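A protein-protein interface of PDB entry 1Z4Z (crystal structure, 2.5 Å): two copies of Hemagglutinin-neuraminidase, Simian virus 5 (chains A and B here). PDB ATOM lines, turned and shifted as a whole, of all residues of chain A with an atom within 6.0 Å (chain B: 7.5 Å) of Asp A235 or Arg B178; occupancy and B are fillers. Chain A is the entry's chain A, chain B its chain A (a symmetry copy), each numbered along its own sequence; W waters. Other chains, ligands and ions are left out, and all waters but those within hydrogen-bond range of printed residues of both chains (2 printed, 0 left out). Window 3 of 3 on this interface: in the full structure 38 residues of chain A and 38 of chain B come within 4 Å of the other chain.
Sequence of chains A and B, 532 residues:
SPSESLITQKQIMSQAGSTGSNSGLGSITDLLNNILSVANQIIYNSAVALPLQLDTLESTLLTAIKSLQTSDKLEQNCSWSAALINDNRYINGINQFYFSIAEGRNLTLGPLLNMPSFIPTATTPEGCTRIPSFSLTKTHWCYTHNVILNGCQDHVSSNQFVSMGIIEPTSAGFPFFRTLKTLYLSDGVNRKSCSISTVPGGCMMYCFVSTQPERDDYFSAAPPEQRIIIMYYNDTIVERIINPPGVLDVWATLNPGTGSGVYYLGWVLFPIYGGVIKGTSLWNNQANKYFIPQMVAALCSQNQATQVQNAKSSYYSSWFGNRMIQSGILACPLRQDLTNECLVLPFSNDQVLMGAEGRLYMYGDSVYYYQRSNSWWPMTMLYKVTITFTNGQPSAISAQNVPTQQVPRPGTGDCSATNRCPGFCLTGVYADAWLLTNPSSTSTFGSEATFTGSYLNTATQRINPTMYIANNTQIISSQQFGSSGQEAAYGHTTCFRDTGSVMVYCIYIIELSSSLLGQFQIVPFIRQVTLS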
ATOM      1  N   LYS A 181     -17.355  28.750  -0.755  1.00  0.00           N
ATOM      2  CA  LYS A 181     -18.518  28.266  -0.024  1.00  0.00           C
ATOM      3  C   LYS A 181     -19.425  29.430   0.317  1.00  0.00           C
ATOM      4  O   LYS A 181     -18.969  30.527   0.619  1.00  0.00           O
ATOM      5  CB  LYS A 181     -18.123  27.549   1.274  1.00  0.00           C
ATOM      6  CG  LYS A 181     -19.314  26.872   1.967  1.00  0.00           C
ATOM      7  CD  LYS A 181     -18.995  26.378   3.384  1.00  0.00           C
ATOM      8  CE  LYS A 181     -17.895  25.335   3.399  1.00  0.00           C
ATOM      9  NZ  LYS A 181     -18.216  24.183   2.516  1.00  0.00           N
ATOM     10  N   THR A 182     -20.718  29.167   0.278  1.00  0.00           N
ATOM     11  CA  THR A 182     -21.726  30.163   0.564  1.00  0.00           C
ATOM     12  C   THR A 182     -22.723  29.542   1.548  1.00  0.00           C
ATOM     13  O   THR A 182     -22.922  28.331   1.547  1.00  0.00           O
ATOM     14  CB  THR A 182     -22.389  30.568  -0.774  1.00  0.00           C
ATOM     15  OG1 THR A 182     -21.841  31.816  -1.213  1.00  0.00           O
ATOM     16  CG2 THR A 182     -23.865  30.662  -0.661  1.00  0.00           C
ATOM     17  N   LEU A 183     -23.309  30.363   2.414  1.00  0.00           N
ATOM     18  CA  LEU A 183     -24.304  29.902   3.384  1.00  0.00           C
ATOM     19  C   LEU A 183     -25.331  30.995   3.570  1.00  0.00           C
ATOM     20  O   LEU A 183     -24.994  32.177   3.550  1.00  0.00           O
ATOM     21  CB  LEU A 183     -23.699  29.624   4.762  1.00  0.00           C
ATOM     22  CG  LEU A 183     -22.564  28.624   4.943  1.00  0.00           C
ATOM     23  CD1 LEU A 183     -21.230  29.320   4.706  1.00  0.00           C
ATOM     24  CD2 LEU A 183     -22.607  28.078   6.355  1.00  0.00           C
ATOM     25  N   TYR A 184     -26.584  30.608   3.773  1.00  0.00           N
ATOM     26  CA  TYR A 184     -27.632  31.590   3.995  1.00  0.00           C
ATOM     27  C   TYR A 184     -28.416  31.146   5.220  1.00  0.00           C
ATOM     28  O   TYR A 184     -29.221  30.217   5.150  1.00  0.00           O
ATOM     29  CB  TYR A 184     -28.542  31.689   2.768  1.00  0.00           C
ATOM     30  CG  TYR A 184     -29.474  32.886   2.746  1.00  0.00           C
ATOM     31  CD1 TYR A 184     -29.022  34.160   3.102  1.00  0.00           C
ATOM     32  CD2 TYR A 184     -30.791  32.757   2.299  1.00  0.00           C
ATOM     33  CE1 TYR A 184     -29.858  35.274   3.007  1.00  0.00           C
ATOM     34  CE2 TYR A 184     -31.636  33.860   2.199  1.00  0.00           C
ATOM     35  CZ  TYR A 184     -31.169  35.115   2.550  1.00  0.00           C
ATOM     36  OH  TYR A 184     -32.012  36.208   2.430  1.00  0.00           O
ATOM     37  N   TYR A 232     -17.413  25.567   9.504  1.00  0.00           N
ATOM     38  CA  TYR A 232     -16.196  24.977   8.971  1.00  0.00           C
ATOM     39  C   TYR A 232     -16.276  24.791   7.468  1.00  0.00           C
ATOM     40  O   TYR A 232     -17.349  24.580   6.905  1.00  0.00           O
ATOM     41  CB  TYR A 232     -15.933  23.630   9.639  1.00  0.00           C
ATOM     42  CG  TYR A 232     -15.607  23.767  11.096  1.00  0.00           C
ATOM     43  CD1 TYR A 232     -14.366  24.236  11.499  1.00  0.00           C
ATOM     44  CD2 TYR A 232     -16.549  23.458  12.079  1.00  0.00           C
ATOM     45  CE1 TYR A 232     -14.059  24.395  12.852  1.00  0.00           C
ATOM     46  CE2 TYR A 232     -16.258  23.616  13.442  1.00  0.00           C
ATOM     47  CZ  TYR A 232     -15.007  24.083  13.819  1.00  0.00           C
ATOM     48  OH  TYR A 232     -14.677  24.234  15.155  1.00  0.00           O
ATOM     49  N   TYR A 233     -15.120  24.873   6.828  1.00  0.00           N
ATOM     50  CA  TYR A 233     -15.016  24.721   5.390  1.00  0.00           C
ATOM     51  C   TYR A 233     -15.500  23.349   4.936  1.00  0.00           C
ATOM     52  O   TYR A 233     -15.823  23.148   3.770  1.00  0.00           O
ATOM     53  CB  TYR A 233     -13.564  24.927   4.962  1.00  0.00           C
ATOM     54  CG  TYR A 233     -13.344  24.831   3.472  1.00  0.00           C
ATOM     55  CD1 TYR A 233     -13.854  25.801   2.598  1.00  0.00           C
ATOM     56  CD2 TYR A 233     -12.607  23.775   2.933  1.00  0.00           C
ATOM     57  CE1 TYR A 233     -13.622  25.715   1.231  1.00  0.00           C
ATOM     58  CE2 TYR A 233     -12.374  23.682   1.569  1.00  0.00           C
ATOM     59  CZ  TYR A 233     -12.878  24.650   0.732  1.00  0.00           C
ATOM     60  OH  TYR A 233     -12.614  24.544  -0.605  1.00  0.00           O
ATOM     61  N   ASN A 234     -15.522  22.397   5.874  1.00  0.00           N
ATOM     62  CA  ASN A 234     -15.987  21.026   5.630  1.00  0.00           C
ATOM     63  C   ASN A 234     -17.504  20.945   5.759  1.00  0.00           C
ATOM     64  O   ASN A 234     -18.067  19.853   5.802  1.00  0.00           O
ATOM     65  CB  ASN A 234     -15.315  19.980   6.553  1.00  0.00           C
ATOM     66  CG  ASN A 234     -15.646  20.153   8.023  1.00  0.00           C
ATOM     67  OD1 ASN A 234     -16.649  20.783   8.389  1.00  0.00           O
ATOM     68  ND2 ASN A 234     -14.790  19.565   8.865  1.00  0.00           N
ATOM     69  N   ASP A 235     -18.149  22.114   5.805  1.00  0.00           N
ATOM     70  CA  ASP A 235     -19.596  22.242   5.915  1.00  0.00           C
ATOM     71  C   ASP A 235     -20.274  21.886   7.236  1.00  0.00           C
ATOM     72  O   ASP A 235     -21.497  21.852   7.308  1.00  0.00           O
ATOM     73  CB  ASP A 235     -20.279  21.512   4.757  1.00  0.00           C
ATOM     74  CG  ASP A 235     -21.128  22.455   3.906  1.00  0.00           C
ATOM     75  OD1 ASP A 235     -20.579  23.470   3.419  1.00  0.00           O
ATOM     76  OD2 ASP A 235     -22.341  22.196   3.730  1.00  0.00           O
ATOM     77  N   THR A 236     -19.497  21.628   8.280  1.00  0.00           N
ATOM     78  CA  THR A 236     -20.087  21.356   9.581  1.00  0.00           C
ATOM     79  C   THR A 236     -20.443  22.728  10.156  1.00  0.00           C
ATOM     80  O   THR A 236     -19.677  23.679  10.006  1.00  0.00           O
ATOM     81  CB  THR A 236     -19.091  20.716  10.574  1.00  0.00           C
ATOM     82  OG1 THR A 236     -18.894  19.340  10.247  1.00  0.00           O
ATOM     83  CG2 THR A 236     -19.626  20.801  12.000  1.00  0.00           C
ATOM     84  N   ILE A 237     -21.605  22.830  10.797  1.00  0.00           N
ATOM     85  CA  ILE A 237     -22.039  24.087  11.397  1.00  0.00           C
ATOM     86  C   ILE A 237     -22.466  23.856  12.837  1.00  0.00           C
ATOM     87  O   ILE A 237     -23.270  22.965  13.125  1.00  0.00           O
ATOM     88  CB  ILE A 237     -23.221  24.701  10.636  1.00  0.00           C
ATOM     89  CG1 ILE A 237     -22.807  25.004   9.199  1.00  0.00           C
ATOM     90  CG2 ILE A 237     -23.679  25.973  11.320  1.00  0.00           C
ATOM     91  CD1 ILE A 237     -23.934  25.553   8.351  1.00  0.00           C
ATOM     92  N   ILE B  85     -25.705  18.658  -3.608  1.00  0.00           N
ATOM     93  CA  ILE B  85     -26.875  18.324  -4.482  1.00  0.00           C
ATOM     94  C   ILE B  85     -28.085  19.197  -4.134  1.00  0.00           C
ATOM     95  O   ILE B  85     -28.189  19.701  -3.021  1.00  0.00           O
ATOM     96  CB  ILE B  85     -27.263  16.839  -4.318  1.00  0.00           C
ATOM     97  CG1 ILE B  85     -28.487  16.517  -5.179  1.00  0.00           C
ATOM     98  CG2 ILE B  85     -27.547  16.540  -2.853  1.00  0.00           C
ATOM     99  CD1 ILE B  85     -28.861  15.063  -5.183  1.00  0.00           C
ATOM    100  N   ASN B  86     -28.996  19.382  -5.086  1.00  0.00           N
ATOM    101  CA  ASN B  86     -30.176  20.207  -4.831  1.00  0.00           C
ATOM    102  C   ASN B  86     -31.020  19.612  -3.717  1.00  0.00           C
ATOM    103  O   ASN B  86     -31.036  18.399  -3.511  1.00  0.00           O
ATOM    104  CB  ASN B  86     -31.042  20.359  -6.088  1.00  0.00           C
ATOM    105  CG  ASN B  86     -30.404  21.254  -7.136  1.00  0.00           C
ATOM    106  OD1 ASN B  86     -29.803  22.276  -6.808  1.00  0.00           O
ATOM    107  ND2 ASN B  86     -30.549  20.882  -8.408  1.00  0.00           N
ATOM    108  N   PRO B 116     -30.331  36.449  -2.272  1.00  0.00           N
ATOM    109  CA  PRO B 116     -28.967  36.929  -2.530  1.00  0.00           C
ATOM    110  C   PRO B 116     -28.583  36.518  -3.948  1.00  0.00           C
ATOM    111  O   PRO B 116     -28.650  35.341  -4.294  1.00  0.00           O
ATOM    112  CB  PRO B 116     -28.135  36.199  -1.480  1.00  0.00           C
ATOM    113  CG  PRO B 116     -29.117  35.982  -0.356  1.00  0.00           C
ATOM    114  CD  PRO B 116     -30.366  35.565  -1.094  1.00  0.00           C
ATOM    115  N   PHE B 118     -26.574  35.328  -7.061  1.00  0.00           N
ATOM    116  CA  PHE B 118     -25.428  34.441  -7.215  1.00  0.00           C
ATOM    117  C   PHE B 118     -24.597  34.854  -8.440  1.00  0.00           C
ATOM    118  O   PHE B 118     -23.643  34.171  -8.816  1.00  0.00           O
ATOM    119  CB  PHE B 118     -25.901  32.986  -7.351  1.00  0.00           C
ATOM    120  CG  PHE B 118     -26.728  32.726  -8.578  1.00  0.00           C
ATOM    121  CD1 PHE B 118     -26.125  32.344  -9.769  1.00  0.00           C
ATOM    122  CD2 PHE B 118     -28.112  32.879  -8.547  1.00  0.00           C
ATOM    123  CE1 PHE B 118     -26.893  32.118 -10.917  1.00  0.00           C
ATOM    124  CE2 PHE B 118     -28.885  32.656  -9.682  1.00  0.00           C
ATOM    125  CZ  PHE B 118     -28.276  32.275 -10.871  1.00  0.00           C
ATOM    126  N   TRP B 141     -26.735  23.399 -10.474  1.00  0.00           N
ATOM    127  CA  TRP B 141     -26.761  24.402 -11.535  1.00  0.00           C
ATOM    128  C   TRP B 141     -25.363  24.920 -11.859  1.00  0.00           C
ATOM    129  O   TRP B 141     -24.471  24.884 -11.018  1.00  0.00           O
ATOM    130  CB  TRP B 141     -27.649  25.588 -11.151  1.00  0.00           C
ATOM    131  CG  TRP B 141     -27.310  26.267  -9.843  1.00  0.00           C
ATOM    132  CD1 TRP B 141     -27.926  26.078  -8.641  1.00  0.00           C
ATOM    133  CD2 TRP B 141     -26.304  27.269  -9.624  1.00  0.00           C
ATOM    134  NE1 TRP B 141     -27.372  26.899  -7.690  1.00  0.00           N
ATOM    135  CE2 TRP B 141     -26.375  27.640  -8.263  1.00  0.00           C
ATOM    136  CE3 TRP B 141     -25.351  27.888 -10.444  1.00  0.00           C
ATOM    137  CZ2 TRP B 141     -25.528  28.607  -7.701  1.00  0.00           C
ATOM    138  CZ3 TRP B 141     -24.502  28.855  -9.885  1.00  0.00           C
ATOM    139  CH2 TRP B 141     -24.599  29.203  -8.525  1.00  0.00           C
ATOM    140  N   SER B 163     -19.485  29.662 -12.167  1.00  0.00           N
ATOM    141  CA  SER B 163     -20.003  29.447 -10.829  1.00  0.00           C
ATOM    142  C   SER B 163     -20.876  28.197 -10.844  1.00  0.00           C
ATOM    143  O   SER B 163     -21.482  27.869 -11.868  1.00  0.00           O
ATOM    144  CB  SER B 163     -20.830  30.669 -10.438  1.00  0.00           C
ATOM    145  OG  SER B 163     -21.339  30.573  -9.136  1.00  0.00           O
ATOM    146  N   MET B 164     -20.932  27.485  -9.727  1.00  0.00           N
ATOM    147  CA  MET B 164     -21.782  26.304  -9.656  1.00  0.00           C
ATOM    148  C   MET B 164     -22.286  26.093  -8.236  1.00  0.00           C
ATOM    149  O   MET B 164     -21.617  26.456  -7.263  1.00  0.00           O
ATOM    150  CB  MET B 164     -21.042  25.062 -10.165  1.00  0.00           C
ATOM    151  CG  MET B 164     -19.913  24.553  -9.300  1.00  0.00           C
ATOM    152  SD  MET B 164     -19.126  23.127 -10.109  1.00  0.00           S
ATOM    153  CE  MET B 164     -18.050  23.962 -11.266  1.00  0.00           C
ATOM    154  N   GLY B 165     -23.479  25.523  -8.121  1.00  0.00           N
ATOM    155  CA  GLY B 165     -24.049  25.292  -6.813  1.00  0.00           C
ATOM    156  C   GLY B 165     -25.352  24.520  -6.836  1.00  0.00           C
ATOM    157  O   GLY B 165     -25.658  23.806  -7.795  1.00  0.00           O
ATOM    158  N   ILE B 166     -26.133  24.689  -5.775  1.00  0.00           N
ATOM    159  CA  ILE B 166     -27.399  23.987  -5.628  1.00  0.00           C
ATOM    160  C   ILE B 166     -28.520  24.933  -5.212  1.00  0.00           C
ATOM    161  O   ILE B 166     -28.284  26.111  -4.947  1.00  0.00           O
ATOM    162  CB  ILE B 166     -27.279  22.900  -4.547  1.00  0.00           C
ATOM    163  CG1 ILE B 166     -27.042  23.570  -3.187  1.00  0.00           C
ATOM    164  CG2 ILE B 166     -26.124  21.953  -4.882  1.00  0.00           C
ATOM    165  CD1 ILE B 166     -26.902  22.616  -2.033  1.00  0.00           C
ATOM    166  N   ILE B 167     -29.738  24.404  -5.138  1.00  0.00           N
ATOM    167  CA  ILE B 167     -30.887  25.202  -4.731  1.00  0.00           C
ATOM    168  C   ILE B 167     -31.428  24.684  -3.409  1.00  0.00           C
ATOM    169  O   ILE B 167     -31.571  23.482  -3.228  1.00  0.00           O
ATOM    170  CB  ILE B 167     -32.038  25.119  -5.740  1.00  0.00           C
ATOM    171  CG1 ILE B 167     -31.545  25.449  -7.141  1.00  0.00           C
ATOM    172  CG2 ILE B 167     -33.135  26.093  -5.341  1.00  0.00           C
ATOM    173  CD1 ILE B 167     -32.593  25.188  -8.209  1.00  0.00           C
ATOM    174  N   GLU B 168     -31.725  25.590  -2.487  1.00  0.00           N
ATOM    175  CA  GLU B 168     -32.275  25.194  -1.200  1.00  0.00           C
ATOM    176  C   GLU B 168     -33.305  26.213  -0.755  1.00  0.00           C
ATOM    177  O   GLU B 168     -33.205  27.392  -1.074  1.00  0.00           O
ATOM    178  CB  GLU B 168     -31.176  25.059  -0.141  1.00  0.00           C
ATOM    179  CG  GLU B 168     -30.410  26.323   0.149  1.00  0.00           C
ATOM    180  CD  GLU B 168     -29.476  26.161   1.337  1.00  0.00           C
ATOM    181  OE1 GLU B 168     -28.809  25.104   1.424  1.00  0.00           O
ATOM    182  OE2 GLU B 168     -29.400  27.091   2.178  1.00  0.00           O
ATOM    183  N   PRO B 175     -36.727  29.811  -3.119  1.00  0.00           N
ATOM    184  CA  PRO B 175     -35.356  29.388  -3.407  1.00  0.00           C
ATOM    185  C   PRO B 175     -34.210  30.340  -3.116  1.00  0.00           C
ATOM    186  O   PRO B 175     -34.359  31.559  -3.136  1.00  0.00           O
ATOM    187  CB  PRO B 175     -35.399  29.046  -4.899  1.00  0.00           C
ATOM    188  CG  PRO B 175     -36.823  28.748  -5.162  1.00  0.00           C
ATOM    189  CD  PRO B 175     -37.527  29.798  -4.356  1.00  0.00           C
ATOM    190  N   PHE B 176     -33.060  29.734  -2.850  1.00  0.00           N
ATOM    191  CA  PHE B 176     -31.812  30.431  -2.626  1.00  0.00           C
ATOM    192  C   PHE B 176     -30.814  29.623  -3.436  1.00  0.00           C
ATOM    193  O   PHE B 176     -30.681  28.421  -3.233  1.00  0.00           O
ATOM    194  CB  PHE B 176     -31.392  30.419  -1.153  1.00  0.00           C
ATOM    195  CG  PHE B 176     -29.917  30.687  -0.942  1.00  0.00           C
ATOM    196  CD1 PHE B 176     -29.283  31.740  -1.604  1.00  0.00           C
ATOM    197  CD2 PHE B 176     -29.157  29.873  -0.108  1.00  0.00           C
ATOM    198  CE1 PHE B 176     -27.921  31.977  -1.443  1.00  0.00           C
ATOM    199  CE2 PHE B 176     -27.790  30.101   0.065  1.00  0.00           C
ATOM    200  CZ  PHE B 176     -27.170  31.156  -0.606  1.00  0.00           C
ATOM    201  N   PHE B 177     -30.144  30.269  -4.378  1.00  0.00           N
ATOM    202  CA  PHE B 177     -29.150  29.590  -5.188  1.00  0.00           C
ATOM    203  C   PHE B 177     -27.831  29.681  -4.457  1.00  0.00           C
ATOM    204  O   PHE B 177     -27.172  30.718  -4.444  1.00  0.00           O
ATOM    205  CB  PHE B 177     -29.067  30.236  -6.564  1.00  0.00           C
ATOM    206  CG  PHE B 177     -30.211  29.873  -7.447  1.00  0.00           C
ATOM    207  CD1 PHE B 177     -31.508  30.268  -7.123  1.00  0.00           C
ATOM    208  CD2 PHE B 177     -30.015  29.086  -8.569  1.00  0.00           C
ATOM    209  CE1 PHE B 177     -32.588  29.879  -7.906  1.00  0.00           C
ATOM    210  CE2 PHE B 177     -31.091  28.692  -9.357  1.00  0.00           C
ATOM    211  CZ  PHE B 177     -32.380  29.090  -9.021  1.00  0.00           C
ATOM    212  N   ARG B 178     -27.469  28.571  -3.831  1.00  0.00           N
ATOM    213  CA  ARG B 178     -26.255  28.478  -3.048  1.00  0.00           C
ATOM    214  C   ARG B 178     -25.023  28.129  -3.883  1.00  0.00           C
ATOM    215  O   ARG B 178     -24.915  27.027  -4.415  1.00  0.00           O
ATOM    216  CB  ARG B 178     -26.450  27.432  -1.953  1.00  0.00           C
ATOM    217  CG  ARG B 178     -25.377  27.450  -0.896  1.00  0.00           C
ATOM    218  CD  ARG B 178     -25.468  26.254  -0.002  1.00  0.00           C
ATOM    219  NE  ARG B 178     -24.384  26.265   0.968  1.00  0.00           N
ATOM    220  CZ  ARG B 178     -24.024  25.220   1.700  1.00  0.00           C
ATOM    221  NH1 ARG B 178     -24.667  24.070   1.568  1.00  0.00           N
ATOM    222  NH2 ARG B 178     -23.019  25.322   2.556  1.00  0.00           N
ATOM    223  N   THR B 179     -24.099  29.079  -3.982  1.00  0.00           N
ATOM    224  CA  THR B 179     -22.870  28.871  -4.731  1.00  0.00           C
ATOM    225  C   THR B 179     -21.942  27.999  -3.901  1.00  0.00           C
ATOM    226  O   THR B 179     -21.654  28.326  -2.749  1.00  0.00           O
ATOM    227  CB  THR B 179     -22.151  30.205  -5.004  1.00  0.00           C
ATOM    228  OG1 THR B 179     -22.987  31.042  -5.814  1.00  0.00           O
ATOM    229  CG2 THR B 179     -20.829  29.964  -5.717  1.00  0.00           C
ATOM    230  N   LEU B 180     -21.481  26.894  -4.483  1.00  0.00           N
ATOM    231  CA  LEU B 180     -20.576  25.985  -3.787  1.00  0.00           C
ATOM    232  C   LEU B 180     -19.159  26.019  -4.356  1.00  0.00           C
ATOM    233  O   LEU B 180     -18.240  25.422  -3.793  1.00  0.00           O
ATOM    234  CB  LEU B 180     -21.106  24.553  -3.838  1.00  0.00           C
ATOM    235  CG  LEU B 180     -22.401  24.277  -3.081  1.00  0.00           C
ATOM    236  CD1 LEU B 180     -22.651  22.779  -3.066  1.00  0.00           C
ATOM    237  CD2 LEU B 180     -22.299  24.813  -1.666  1.00  0.00           C
ATOM    238  N   LYS B 181     -18.986  26.706  -5.480  1.00  0.00           N
ATOM    239  CA  LYS B 181     -17.675  26.826  -6.104  1.00  0.00           C
ATOM    240  C   LYS B 181     -17.694  27.952  -7.116  1.00  0.00           C
ATOM    241  O   LYS B 181     -18.684  28.175  -7.805  1.00  0.00           O
ATOM    242  CB  LYS B 181     -17.255  25.530  -6.813  1.00  0.00           C
ATOM    243  CG  LYS B 181     -15.807  25.570  -7.320  1.00  0.00           C
ATOM    244  CD  LYS B 181     -15.453  24.402  -8.249  1.00  0.00           C
ATOM    245  CE  LYS B 181     -15.588  23.056  -7.564  1.00  0.00           C
ATOM    246  NZ  LYS B 181     -14.772  22.986  -6.323  1.00  0.00           N
ATOM    247  N   TYR B 233     -16.686  19.374  -9.779  1.00  0.00           N
ATOM    248  CA  TYR B 233     -16.937  19.890  -8.447  1.00  0.00           C
ATOM    249  C   TYR B 233     -15.778  19.592  -7.503  1.00  0.00           C
ATOM    250  O   TYR B 233     -15.630  20.228  -6.465  1.00  0.00           O
ATOM    251  CB  TYR B 233     -18.223  19.274  -7.899  1.00  0.00           C
ATOM    252  CG  TYR B 233     -18.606  19.772  -6.527  1.00  0.00           C
ATOM    253  CD1 TYR B 233     -19.024  21.096  -6.325  1.00  0.00           C
ATOM    254  CD2 TYR B 233     -18.568  18.914  -5.427  1.00  0.00           C
ATOM    255  CE1 TYR B 233     -19.399  21.534  -5.061  1.00  0.00           C
ATOM    256  CE2 TYR B 233     -18.939  19.347  -4.163  1.00  0.00           C
ATOM    257  CZ  TYR B 233     -19.353  20.647  -3.990  1.00  0.00           C
ATOM    258  OH  TYR B 233     -19.733  21.039  -2.738  1.00  0.00           O
HETATM  259  O   HOH W   1     -31.004  28.564   3.789  1.00  0.00           O
HETATM  260  O   HOH W   2     -27.112  27.481   3.637  1.00  0.00           O
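The backbone carbonyl oxygen (O) of Thr A182 is in hydrogen-bond range of the guanidinium group (NE) of Arg B178.
O of Thr B179 sits close to N of Thr A182 (3.3 Å).
OD1 of Asp A235 lies within salt-bridge range of NH2 of Arg B178.
NZ of Lys A181 lies within hydrogen-bond range of O of Tyr A233 (2.9 Å).
NZ of Lys A181 is in salt-bridge range of OD1 of Asp A235.
The backbone carbonyl oxygen (O) of Ile B166 sits at hydrogen-bond distance from the backbone NH (N) of Arg B178, 2.8 Å away.
The backbone NH (N) of Phe B176 sits at hydrogen-bond distance from the backbone carbonyl oxygen (O) of Glu B168 (2.9 Å).
Among the printed residues, pairs that only touch across the chains: Lys A181 with Thr B179 (3.9 Å), Thr A182 with Phe B176 (3.3 Å), Tyr A184 with Pro B116 (3.5 Å) and Tyr A184 with Phe B176 (3.2 Å).
Asp A235 touches just one residue of chain B: Arg B178 (3.2 Å).
Printed residues of chain A within 4 Å of Arg B178: Thr A182 and Asp A235.
Of the printed residues of chain B, Thr A182 touches Phe B176 (3.3 Å), Arg B178 (2.6 Å) and Thr B179 (3.1 Å).
Of the printed residues of chain B, Tyr A184 touches Pro B116 and Phe B176.
Of the printed residues of chain A, Phe B176 touches Thr A182 (3.3 Å) and Tyr A184 (3.2 Å).
Phe B177 touches none of the printed residues of chain A.
The nearest residue of chain B that does not touch Asp A235 is Leu B180 (5.5 Å).
The nearest printed residue of chain A that does not touch Phe B176 is Leu A183 (4.4 Å).
Printed residues of chain B that touch a printed residue of chain A: Pro B116, Phe B176, Arg B178 and Thr B179.
Hydrophobic or aromatic side chains of chain B within 4 Å of the printed part of chain A: Pro B116 and Phe B176.
Of the 10 printed residues of chain A, 4 touch a printed residue of chain B.
Among the printed residues, Asp or Glu carboxylates within 4 Å of a Lys or Arg side-chain nitrogen of the other chain: Asp A235 with Arg B178 (3.2 Å).
2 positions are printed for both chains.
Of the 7 pairs that touch across the chains among the printed residues, none has its exchanged pair printed and touching as well.
Water W1 lies within hydrogen-bond range of the side-chain carboxylate (OE2) of Glu B168 (2.7 Å) and the backbone carbonyl oxygen (O) of Tyr A184 (2.8 Å).
Water W2 bridges the side-chain carboxylate of Glu B168 (2.7 Å) and the backbone NH of Tyr A184 (3.2 Å).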
